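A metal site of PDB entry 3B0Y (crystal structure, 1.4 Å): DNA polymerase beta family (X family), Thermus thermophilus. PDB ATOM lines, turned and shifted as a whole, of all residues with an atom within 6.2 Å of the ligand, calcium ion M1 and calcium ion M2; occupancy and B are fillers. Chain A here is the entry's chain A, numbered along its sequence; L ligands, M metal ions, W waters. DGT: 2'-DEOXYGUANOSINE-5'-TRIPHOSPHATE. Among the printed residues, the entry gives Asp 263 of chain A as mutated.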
ATOM      1  N   ARG A 157      -2.525  11.541  -0.633  1.00  0.00           N
ATOM      2  CA  ARG A 157      -2.628  12.351   0.589  1.00  0.00           C
ATOM      3  C   ARG A 157      -1.997  11.578   1.741  1.00  0.00           C
ATOM      4  O   ARG A 157      -1.967  10.341   1.744  1.00  0.00           O
ATOM      5  CB  ARG A 157      -4.094  12.694   0.861  1.00  0.00           C
ATOM      6  CG  ARG A 157      -4.755  13.338  -0.366  1.00  0.00           C
ATOM      7  CD  ARG A 157      -6.176  13.797  -0.110  1.00  0.00           C
ATOM      8  NE  ARG A 157      -6.269  14.900   0.857  1.00  0.00           N
ATOM      9  CZ  ARG A 157      -6.074  16.184   0.577  1.00  0.00           C
ATOM     10  NH1 ARG A 157      -5.822  16.577  -0.674  1.00  0.00           N
ATOM     11  NH2 ARG A 157      -6.189  17.077   1.534  1.00  0.00           N
ATOM     12  N   CYS A 186       0.637  27.123   5.778  1.00  0.00           N
ATOM     13  CA  CYS A 186      -0.743  27.438   5.400  1.00  0.00           C
ATOM     14  C   CYS A 186      -1.427  26.218   4.760  1.00  0.00           C
ATOM     15  O   CYS A 186      -1.244  25.113   5.254  1.00  0.00           O
ATOM     16  CB  CYS A 186      -0.795  28.691   4.529  1.00  0.00           C
ATOM     17  SG  CYS A 186      -0.161  30.188   5.359  1.00  0.00           S
ATOM     18  N   GLY A 187      -2.203  26.425   3.705  1.00  0.00           N
ATOM     19  CA  GLY A 187      -2.966  25.365   3.062  1.00  0.00           C
ATOM     20  C   GLY A 187      -3.838  24.582   4.027  1.00  0.00           C
ATOM     21  O   GLY A 187      -4.240  25.035   5.118  1.00  0.00           O
ATOM     22  N   SER A 188      -4.152  23.356   3.615  1.00  0.00           N
ATOM     23  CA  SER A 188      -5.054  22.516   4.410  1.00  0.00           C
ATOM     24  C   SER A 188      -4.479  22.092   5.749  1.00  0.00           C
ATOM     25  O   SER A 188      -5.238  21.852   6.703  1.00  0.00           O
ATOM     26  CB  SER A 188      -5.488  21.297   3.593  1.00  0.00           C
ATOM     27  OG  SER A 188      -4.322  20.534   3.295  1.00  0.00           O
ATOM     28  N   ALA A 189      -3.156  22.094   5.868  1.00  0.00           N
ATOM     29  CA  ALA A 189      -2.542  21.790   7.161  1.00  0.00           C
ATOM     30  C   ALA A 189      -2.954  22.824   8.212  1.00  0.00           C
ATOM     31  O   ALA A 189      -3.215  22.494   9.368  1.00  0.00           O
ATOM     32  CB  ALA A 189      -1.014  21.764   7.065  1.00  0.00           C
ATOM     33  N   ARG A 191      -5.625  24.417   8.337  1.00  0.00           N
ATOM     34  CA  ARG A 191      -7.049  24.176   8.622  1.00  0.00           C
ATOM     35  C   ARG A 191      -7.270  22.863   9.411  1.00  0.00           C
ATOM     36  O   ARG A 191      -8.405  22.543   9.716  1.00  0.00           O
ATOM     37  CB  ARG A 191      -7.879  24.183   7.341  1.00  0.00           C
ATOM     38  CG  ARG A 191      -7.628  25.399   6.446  1.00  0.00           C
ATOM     39  CD  ARG A 191      -8.771  25.633   5.438  1.00  0.00           C
ATOM     40  NE  ARG A 191      -9.053  24.420   4.666  1.00  0.00           N
ATOM     41  CZ  ARG A 191      -8.429  24.048   3.554  1.00  0.00           C
ATOM     42  NH1 ARG A 191      -7.420  24.766   3.030  1.00  0.00           N
ATOM     43  NH2 ARG A 191      -8.788  22.915   2.933  1.00  0.00           N
ATOM     44  N   LYS A 193      -7.073  19.841   8.463  1.00  0.00           N
ATOM     45  CA  LYS A 193      -7.666  18.753   7.673  1.00  0.00           C
ATOM     46  C   LYS A 193      -6.922  17.465   7.973  1.00  0.00           C
ATOM     47  O   LYS A 193      -5.690  17.482   8.114  1.00  0.00           O
ATOM     48  CB  LYS A 193      -7.587  19.123   6.201  1.00  0.00           C
ATOM     49  CG  LYS A 193      -8.488  18.248   5.329  1.00  0.00           C
ATOM     50  CD  LYS A 193      -8.410  18.726   3.897  1.00  0.00           C
ATOM     51  CE  LYS A 193      -9.262  17.868   2.971  1.00  0.00           C
ATOM     52  NZ  LYS A 193     -10.700  18.146   3.229  1.00  0.00           N
ATOM     53  N   THR A 195      -6.166  14.756   6.331  1.00  0.00           N
ATOM     54  CA  THR A 195      -5.184  14.313   5.318  1.00  0.00           C
ATOM     55  C   THR A 195      -4.859  15.526   4.500  1.00  0.00           C
ATOM     56  O   THR A 195      -5.716  16.405   4.303  1.00  0.00           O
ATOM     57  CB  THR A 195      -5.649  13.160   4.413  1.00  0.00           C
ATOM     58  OG1 THR A 195      -6.685  13.614   3.546  1.00  0.00           O
ATOM     59  CG2 THR A 195      -6.146  11.976   5.278  1.00  0.00           C
ATOM     60  N   VAL A 196      -3.623  15.578   4.029  1.00  0.00           N
ATOM     61  CA  VAL A 196      -3.129  16.741   3.283  1.00  0.00           C
ATOM     62  C   VAL A 196      -2.479  16.322   1.988  1.00  0.00           C
ATOM     63  O   VAL A 196      -1.879  15.228   1.898  1.00  0.00           O
ATOM     64  CB  VAL A 196      -2.172  17.619   4.110  1.00  0.00           C
ATOM     65  CG1 VAL A 196      -2.933  18.170   5.337  1.00  0.00           C
ATOM     66  CG2 VAL A 196      -0.913  16.824   4.505  1.00  0.00           C
ATOM     67  N   GLY A 197      -2.570  17.187   0.987  1.00  0.00           N
ATOM     68  CA  GLY A 197      -1.770  17.027  -0.231  1.00  0.00           C
ATOM     69  C   GLY A 197      -0.430  17.700   0.000  1.00  0.00           C
ATOM     70  O   GLY A 197       0.252  17.466   1.003  1.00  0.00           O
ATOM     71  N   ASP A 198      -0.028  18.542  -0.935  1.00  0.00           N
ATOM     72  CA  ASP A 198       1.230  19.246  -0.750  1.00  0.00           C
ATOM     73  C   ASP A 198       1.162  20.216   0.450  1.00  0.00           C
ATOM     74  O   ASP A 198       0.061  20.568   0.919  1.00  0.00           O
ATOM     75  CB  ASP A 198       1.702  19.949  -2.043  1.00  0.00           C
ATOM     76  CG  ASP A 198       0.815  21.095  -2.470  1.00  0.00           C
ATOM     77  OD1 ASP A 198      -0.009  21.615  -1.697  1.00  0.00           O
ATOM     78  OD2 ASP A 198       0.946  21.533  -3.629  1.00  0.00           O
ATOM     79  N   LEU A 199       2.334  20.618   0.933  1.00  0.00           N
ATOM     80  CA  LEU A 199       2.418  21.590   2.026  1.00  0.00           C
ATOM     81  C   LEU A 199       2.726  22.956   1.442  1.00  0.00           C
ATOM     82  O   LEU A 199       3.485  23.051   0.506  1.00  0.00           O
ATOM     83  CB  LEU A 199       3.517  21.183   3.004  1.00  0.00           C
ATOM     84  CG  LEU A 199       3.181  19.896   3.765  1.00  0.00           C
ATOM     85  CD1 LEU A 199       4.412  19.298   4.375  1.00  0.00           C
ATOM     86  CD2 LEU A 199       2.086  20.086   4.775  1.00  0.00           C
ATOM     87  N   ASP A 200       2.120  24.000   2.001  1.00  0.00           N
ATOM     88  CA  ASP A 200       2.197  25.339   1.422  1.00  0.00           C
ATOM     89  C   ASP A 200       2.681  26.306   2.494  1.00  0.00           C
ATOM     90  O   ASP A 200       2.111  26.340   3.592  1.00  0.00           O
ATOM     91  CB  ASP A 200       0.783  25.768   1.001  1.00  0.00           C
ATOM     92  CG  ASP A 200       0.153  24.760   0.103  1.00  0.00           C
ATOM     93  OD1 ASP A 200       0.415  24.820  -1.117  1.00  0.00           O
ATOM     94  OD2 ASP A 200      -0.574  23.873   0.629  1.00  0.00           O
ATOM     95  N   ASP A 243       5.121  23.852  -1.645  1.00  0.00           N
ATOM     96  CA  ASP A 243       4.963  25.098  -2.355  1.00  0.00           C
ATOM     97  C   ASP A 243       5.322  26.247  -1.411  1.00  0.00           C
ATOM     98  O   ASP A 243       4.942  26.246  -0.237  1.00  0.00           O
ATOM     99  CB  ASP A 243       3.510  25.297  -2.761  1.00  0.00           C
ATOM    100  CG  ASP A 243       3.072  24.424  -3.920  1.00  0.00           C
ATOM    101  OD1 ASP A 243       3.903  23.899  -4.664  1.00  0.00           O
ATOM    102  OD2 ASP A 243       1.845  24.317  -4.090  1.00  0.00           O
ATOM    103  N   GLN A 257      -4.364  34.672   4.314  1.00  0.00           N
ATOM    104  CA  GLN A 257      -5.726  34.293   3.966  1.00  0.00           C
ATOM    105  C   GLN A 257      -5.709  33.523   2.628  1.00  0.00           C
ATOM    106  O   GLN A 257      -6.304  32.426   2.492  1.00  0.00           O
ATOM    107  CB  GLN A 257      -6.601  35.531   3.891  1.00  0.00           C
ATOM    108  CG  GLN A 257      -8.095  35.202   3.797  1.00  0.00           C
ATOM    109  CD  GLN A 257      -8.492  34.736   2.396  1.00  0.00           C
ATOM    110  OE1 GLN A 257      -8.151  35.353   1.384  1.00  0.00           O
ATOM    111  NE2 GLN A 257      -9.209  33.624   2.338  1.00  0.00           N
ATOM    112  N   TYR A 258      -5.014  34.077   1.635  1.00  0.00           N
ATOM    113  CA  TYR A 258      -4.992  33.480   0.303  1.00  0.00           C
ATOM    114  C   TYR A 258      -4.508  32.033   0.372  1.00  0.00           C
ATOM    115  O   TYR A 258      -5.109  31.131  -0.231  1.00  0.00           O
ATOM    116  CB  TYR A 258      -4.063  34.315  -0.591  1.00  0.00           C
ATOM    117  CG  TYR A 258      -3.843  33.723  -1.954  1.00  0.00           C
ATOM    118  CD1 TYR A 258      -4.687  34.045  -3.006  1.00  0.00           C
ATOM    119  CD2 TYR A 258      -2.816  32.814  -2.168  1.00  0.00           C
ATOM    120  CE1 TYR A 258      -4.499  33.488  -4.258  1.00  0.00           C
ATOM    121  CE2 TYR A 258      -2.606  32.263  -3.427  1.00  0.00           C
ATOM    122  CZ  TYR A 258      -3.452  32.584  -4.459  1.00  0.00           C
ATOM    123  OH  TYR A 258      -3.276  32.019  -5.703  1.00  0.00           O
ATOM    124  N   LEU A 259      -3.373  31.829   1.029  1.00  0.00           N
ATOM    125  CA  LEU A 259      -2.725  30.537   0.976  1.00  0.00           C
ATOM    126  C   LEU A 259      -3.351  29.502   1.922  1.00  0.00           C
ATOM    127  O   LEU A 259      -3.035  28.322   1.827  1.00  0.00           O
ATOM    128  CB  LEU A 259      -1.220  30.717   1.199  1.00  0.00           C
ATOM    129  CG  LEU A 259      -0.384  29.526   0.719  1.00  0.00           C
ATOM    130  CD1 LEU A 259      -0.658  29.150  -0.693  1.00  0.00           C
ATOM    131  CD2 LEU A 259       1.099  29.716   0.981  1.00  0.00           C
ATOM    132  N   THR A 260      -4.188  29.967   2.851  1.00  0.00           N
ATOM    133  CA  THR A 260      -4.860  29.056   3.783  1.00  0.00           C
ATOM    134  C   THR A 260      -6.163  28.527   3.206  1.00  0.00           C
ATOM    135  O   THR A 260      -6.562  27.405   3.501  1.00  0.00           O
ATOM    136  CB  THR A 260      -5.103  29.778   5.136  1.00  0.00           C
ATOM    137  OG1 THR A 260      -3.811  30.096   5.693  1.00  0.00           O
ATOM    138  CG2 THR A 260      -5.868  28.888   6.132  1.00  0.00           C
ATOM    139  N   GLY A 261      -6.843  29.335   2.385  1.00  0.00           N
ATOM    140  CA  GLY A 261      -8.112  28.930   1.822  1.00  0.00           C
ATOM    141  C   GLY A 261      -9.098  28.536   2.912  1.00  0.00           C
ATOM    142  O   GLY A 261      -9.111  29.129   3.983  1.00  0.00           O
ATOM    143  N   SER A 262      -9.938  27.516   2.699  1.00  0.00           N
ATOM    144  CA  SER A 262     -10.075  26.777   1.449  1.00  0.00           C
ATOM    145  C   SER A 262     -10.438  27.702   0.297  1.00  0.00           C
ATOM    146  O   SER A 262     -10.847  28.869   0.492  1.00  0.00           O
ATOM    147  CB  SER A 262     -11.181  25.756   1.634  1.00  0.00           C
ATOM    148  OG  SER A 262     -12.443  26.418   1.712  1.00  0.00           O
ATOM    149  N   ASP A 263     -10.338  27.179  -0.921  1.00  0.00           N
ATOM    150  CA  ASP A 263     -10.726  27.926  -2.092  1.00  0.00           C
ATOM    151  C   ASP A 263     -12.178  28.401  -1.918  1.00  0.00           C
ATOM    152  O   ASP A 263     -12.490  29.559  -2.198  1.00  0.00           O
ATOM    153  CB  ASP A 263     -10.578  27.037  -3.327  1.00  0.00           C
ATOM    154  CG  ASP A 263     -10.771  27.790  -4.620  1.00  0.00           C
ATOM    155  OD1 ASP A 263     -10.289  28.929  -4.754  1.00  0.00           O
ATOM    156  OD2 ASP A 263     -11.416  27.205  -5.512  1.00  0.00           O
ATOM    157  N   SER A 266     -12.326  31.414   0.344  1.00  0.00           N
ATOM    158  CA  SER A 266     -11.773  32.613  -0.281  1.00  0.00           C
ATOM    159  C   SER A 266     -12.745  33.156  -1.336  1.00  0.00           C
ATOM    160  O   SER A 266     -12.873  34.366  -1.482  1.00  0.00           O
ATOM    161  CB  SER A 266     -10.448  32.287  -0.928  1.00  0.00           C
ATOM    162  OG  SER A 266      -9.517  31.913   0.057  1.00  0.00           O
HETATM  163  PG  DGT L   1      -4.618  20.018  -0.290  1.00  0.00           P
HETATM  164  O1G DGT L   1      -3.243  20.451  -0.743  1.00  0.00           O
HETATM  165  O2G DGT L   1      -5.419  19.265  -1.333  1.00  0.00           O
HETATM  166  O3G DGT L   1      -4.568  19.279   1.041  1.00  0.00           O
HETATM  167  O3B DGT L   1      -5.473  21.361   0.050  1.00  0.00           O
HETATM  168  PB  DGT L   1      -5.014  22.889   0.060  1.00  0.00           P
HETATM  169  O1B DGT L   1      -6.156  23.697   0.556  1.00  0.00           O
HETATM  170  O2B DGT L   1      -3.660  23.051   0.720  1.00  0.00           O
HETATM  171  O3A DGT L   1      -4.879  23.247  -1.499  1.00  0.00           O
HETATM  172  PA  DGT L   1      -3.691  23.721  -2.471  1.00  0.00           P
HETATM  173  O1A DGT L   1      -2.361  23.268  -1.949  1.00  0.00           O
HETATM  174  O2A DGT L   1      -4.100  23.296  -3.850  1.00  0.00           O
HETATM  175  O5' DGT L   1      -3.799  25.288  -2.442  1.00  0.00           O
HETATM  176  C5' DGT L   1      -3.429  25.997  -1.243  1.00  0.00           C
HETATM  177  C4' DGT L   1      -4.368  27.177  -1.047  1.00  0.00           C
HETATM  178  O4' DGT L   1      -4.203  28.045  -2.164  1.00  0.00           O
HETATM  179  C3' DGT L   1      -5.860  26.847  -1.040  1.00  0.00           C
HETATM  180  O3' DGT L   1      -6.343  26.485   0.242  1.00  0.00           O
HETATM  181  C2' DGT L   1      -6.506  28.161  -1.480  1.00  0.00           C
HETATM  182  C1' DGT L   1      -5.423  28.801  -2.366  1.00  0.00           C
HETATM  183  N9  DGT L   1      -5.798  28.723  -3.792  1.00  0.00           N
HETATM  184  C8  DGT L   1      -5.524  29.642  -4.732  1.00  0.00           C
HETATM  185  N7  DGT L   1      -6.004  29.242  -5.934  1.00  0.00           N
HETATM  186  C5  DGT L   1      -6.601  28.052  -5.775  1.00  0.00           C
HETATM  187  C6  DGT L   1      -7.318  27.078  -6.638  1.00  0.00           C
HETATM  188  O6  DGT L   1      -7.475  27.294  -7.865  1.00  0.00           O
HETATM  189  N1  DGT L   1      -7.801  25.953  -6.069  1.00  0.00           N
HETATM  190  C2  DGT L   1      -7.655  25.669  -4.759  1.00  0.00           C
HETATM  191  N2  DGT L   1      -8.171  24.515  -4.237  1.00  0.00           N
HETATM  192  N3  DGT L   1      -7.010  26.528  -3.934  1.00  0.00           N
HETATM  193  C4  DGT L   1      -6.477  27.700  -4.373  1.00  0.00           C
HETATM  194 CA    CA M   1      -0.180  23.668  -3.103  1.00  0.00          CA
HETATM  195 CA    CA M   2      -1.673  21.978  -0.020  1.00  0.00          CA
HETATM  196  O   HOH W   1      -4.349  25.162  -5.936  1.00  0.00           O
HETATM  197  O   HOH W   2      -1.902  21.408   2.438  1.00  0.00           O
HETATM  198  O   HOH W   3      -9.580  24.483  -1.371  1.00  0.00           O
HETATM  199  O   HOH W   4      -8.640  22.402   0.219  1.00  0.00           O
HETATM  200  O   HOH W   5      -2.111  19.297  -2.945  1.00  0.00           O
HETATM  201  O   HOH W   6      -8.193  19.695  -0.878  1.00  0.00           O
HETATM  202  O   HOH W   7      -5.653  19.194  -4.025  1.00  0.00           O
HETATM  203  O   HOH W   8      -7.426  31.458  -1.556  1.00  0.00           O
HETATM  204  O   HOH W   9      -0.887  25.833  -3.906  1.00  0.00           O
HETATM  205  O   HOH W  10      -3.069  27.351  -4.739  1.00  0.00           O
HETATM  206  O   HOH W  11      -1.399  22.974  -5.059  1.00  0.00           O
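Within 4 Å of calcium ion M1: Asp 198, Asp 200 and Asp 243. The nearest printed residue that does not touch calcium ion M1 is Leu 199 (5.2 Å).
CA of Gly 187 touches O2B of the ligand, at 3.4 Å. CA of Val 196 touches O3G of the ligand, 3.7 Å away. O of Tyr 258 touches C1' of the ligand (3.2 Å). Leu 259 touches the ligand. Gly 261 touches the ligand. Ser 262 touches the ligand (CA to O3', 3.9 Å). Asp 263 touches the ligand. 14 residues have an atom within 4 Å of the ligand: Arg 157, Gly 187, Ser 188, Arg 191, Val 196, Gly 197, Asp 198, Asp 200, Tyr 258, Leu 259, Thr 260, Gly 261, Ser 262 and Asp 263.
Water W4 bridges NH2 of Arg 191 (2.8 Å) and O1B of the ligand (2.8 Å). Water W3 lies within hydrogen-bond range of N of Asp 263 (2.8 Å) and N2 of the ligand (3.2 Å). Water W8 lies within hydrogen-bond range of OG of Ser 266 (2.7 Å) and O of Tyr 258 (2.7 Å).
Calcium ion M2 is bound by OD2 of Asp 200 (2.3 Å), O1G of the ligand (2.3 Å), O2B of the ligand (2.4 Å), OD1 of Asp 198 (2.4 Å), O1A of the ligand (2.4 Å), O of Asp 198 (2.4 Å) and water W2 (2.5 Å).
O of Ser 262 sits at hydrogen-bond distance from OG of Ser 266 (3.4 Å). NH1 of Arg 191 is in hydrogen-bond range of O of Thr 260 (2.8 Å). The backbone NH (N) of Lys 193 sits at hydrogen-bond distance from the backbone carbonyl oxygen (O) of Ser 188, 3.2 Å away. The backbone NH (N) of Gly 187 lies within hydrogen-bond range of the backbone carbonyl oxygen (O) of Leu 259 (2.8 Å). NH2 of Arg 157 lies within hydrogen-bond range of O of Thr 195 (2.9 Å). The side-chain hydroxyl of Thr 260 sits close to the side-chain sulfur of Cys 186 (3.7 Å). The backbone NH (N) of Asp 243 sits at hydrogen-bond distance from the backbone carbonyl oxygen (O) of Leu 199. The backbone carbonyl oxygen (O) of Asp 200 is in hydrogen-bond range of the backbone NH (N) of Cys 186 (2.8 Å).
Calcium ion M1 is bound by the side-chain carboxylate (OD2) of Asp 243 (2.3 Å), the side-chain carboxylate (OD1) of Asp 200 (2.4 Å), water W11 (2.4 Å), water W9 (2.4 Å), the side-chain carboxylate (OD2) of Asp 198 (2.5 Å), the side-chain carboxylate (OD1) of Asp 198 (2.5 Å) and an oxygen (O1A) of the ligand (2.5 Å). Calcium ion M1 has seven donor atoms within binding distance.
Within 4 Å of calcium ion M2: Asp 198 and Asp 200.
The backbone carbonyl oxygen (O) of Thr 260 sits at hydrogen-bond distance from an oxygen (O3') of the ligand (3.4 Å). An oxygen (O3G) of the ligand is in hydrogen-bond range of the side-chain hydroxyl of Ser 188. An oxygen (O2B) of the ligand lies close to the backbone NH (N) of Ser 188 (3.0 Å). The guanidinium group (NH1) of Arg 191 lies within salt-bridge range of an oxygen (O1B) of the ligand. The guanidinium group (NH2) of Arg 157 is in salt-bridge range of an oxygen (O3G) of the ligand (2.8 Å). The backbone NH of Gly 197 lies within hydrogen-bond range of an oxygen (O3G) of the ligand, at 2.9 Å.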
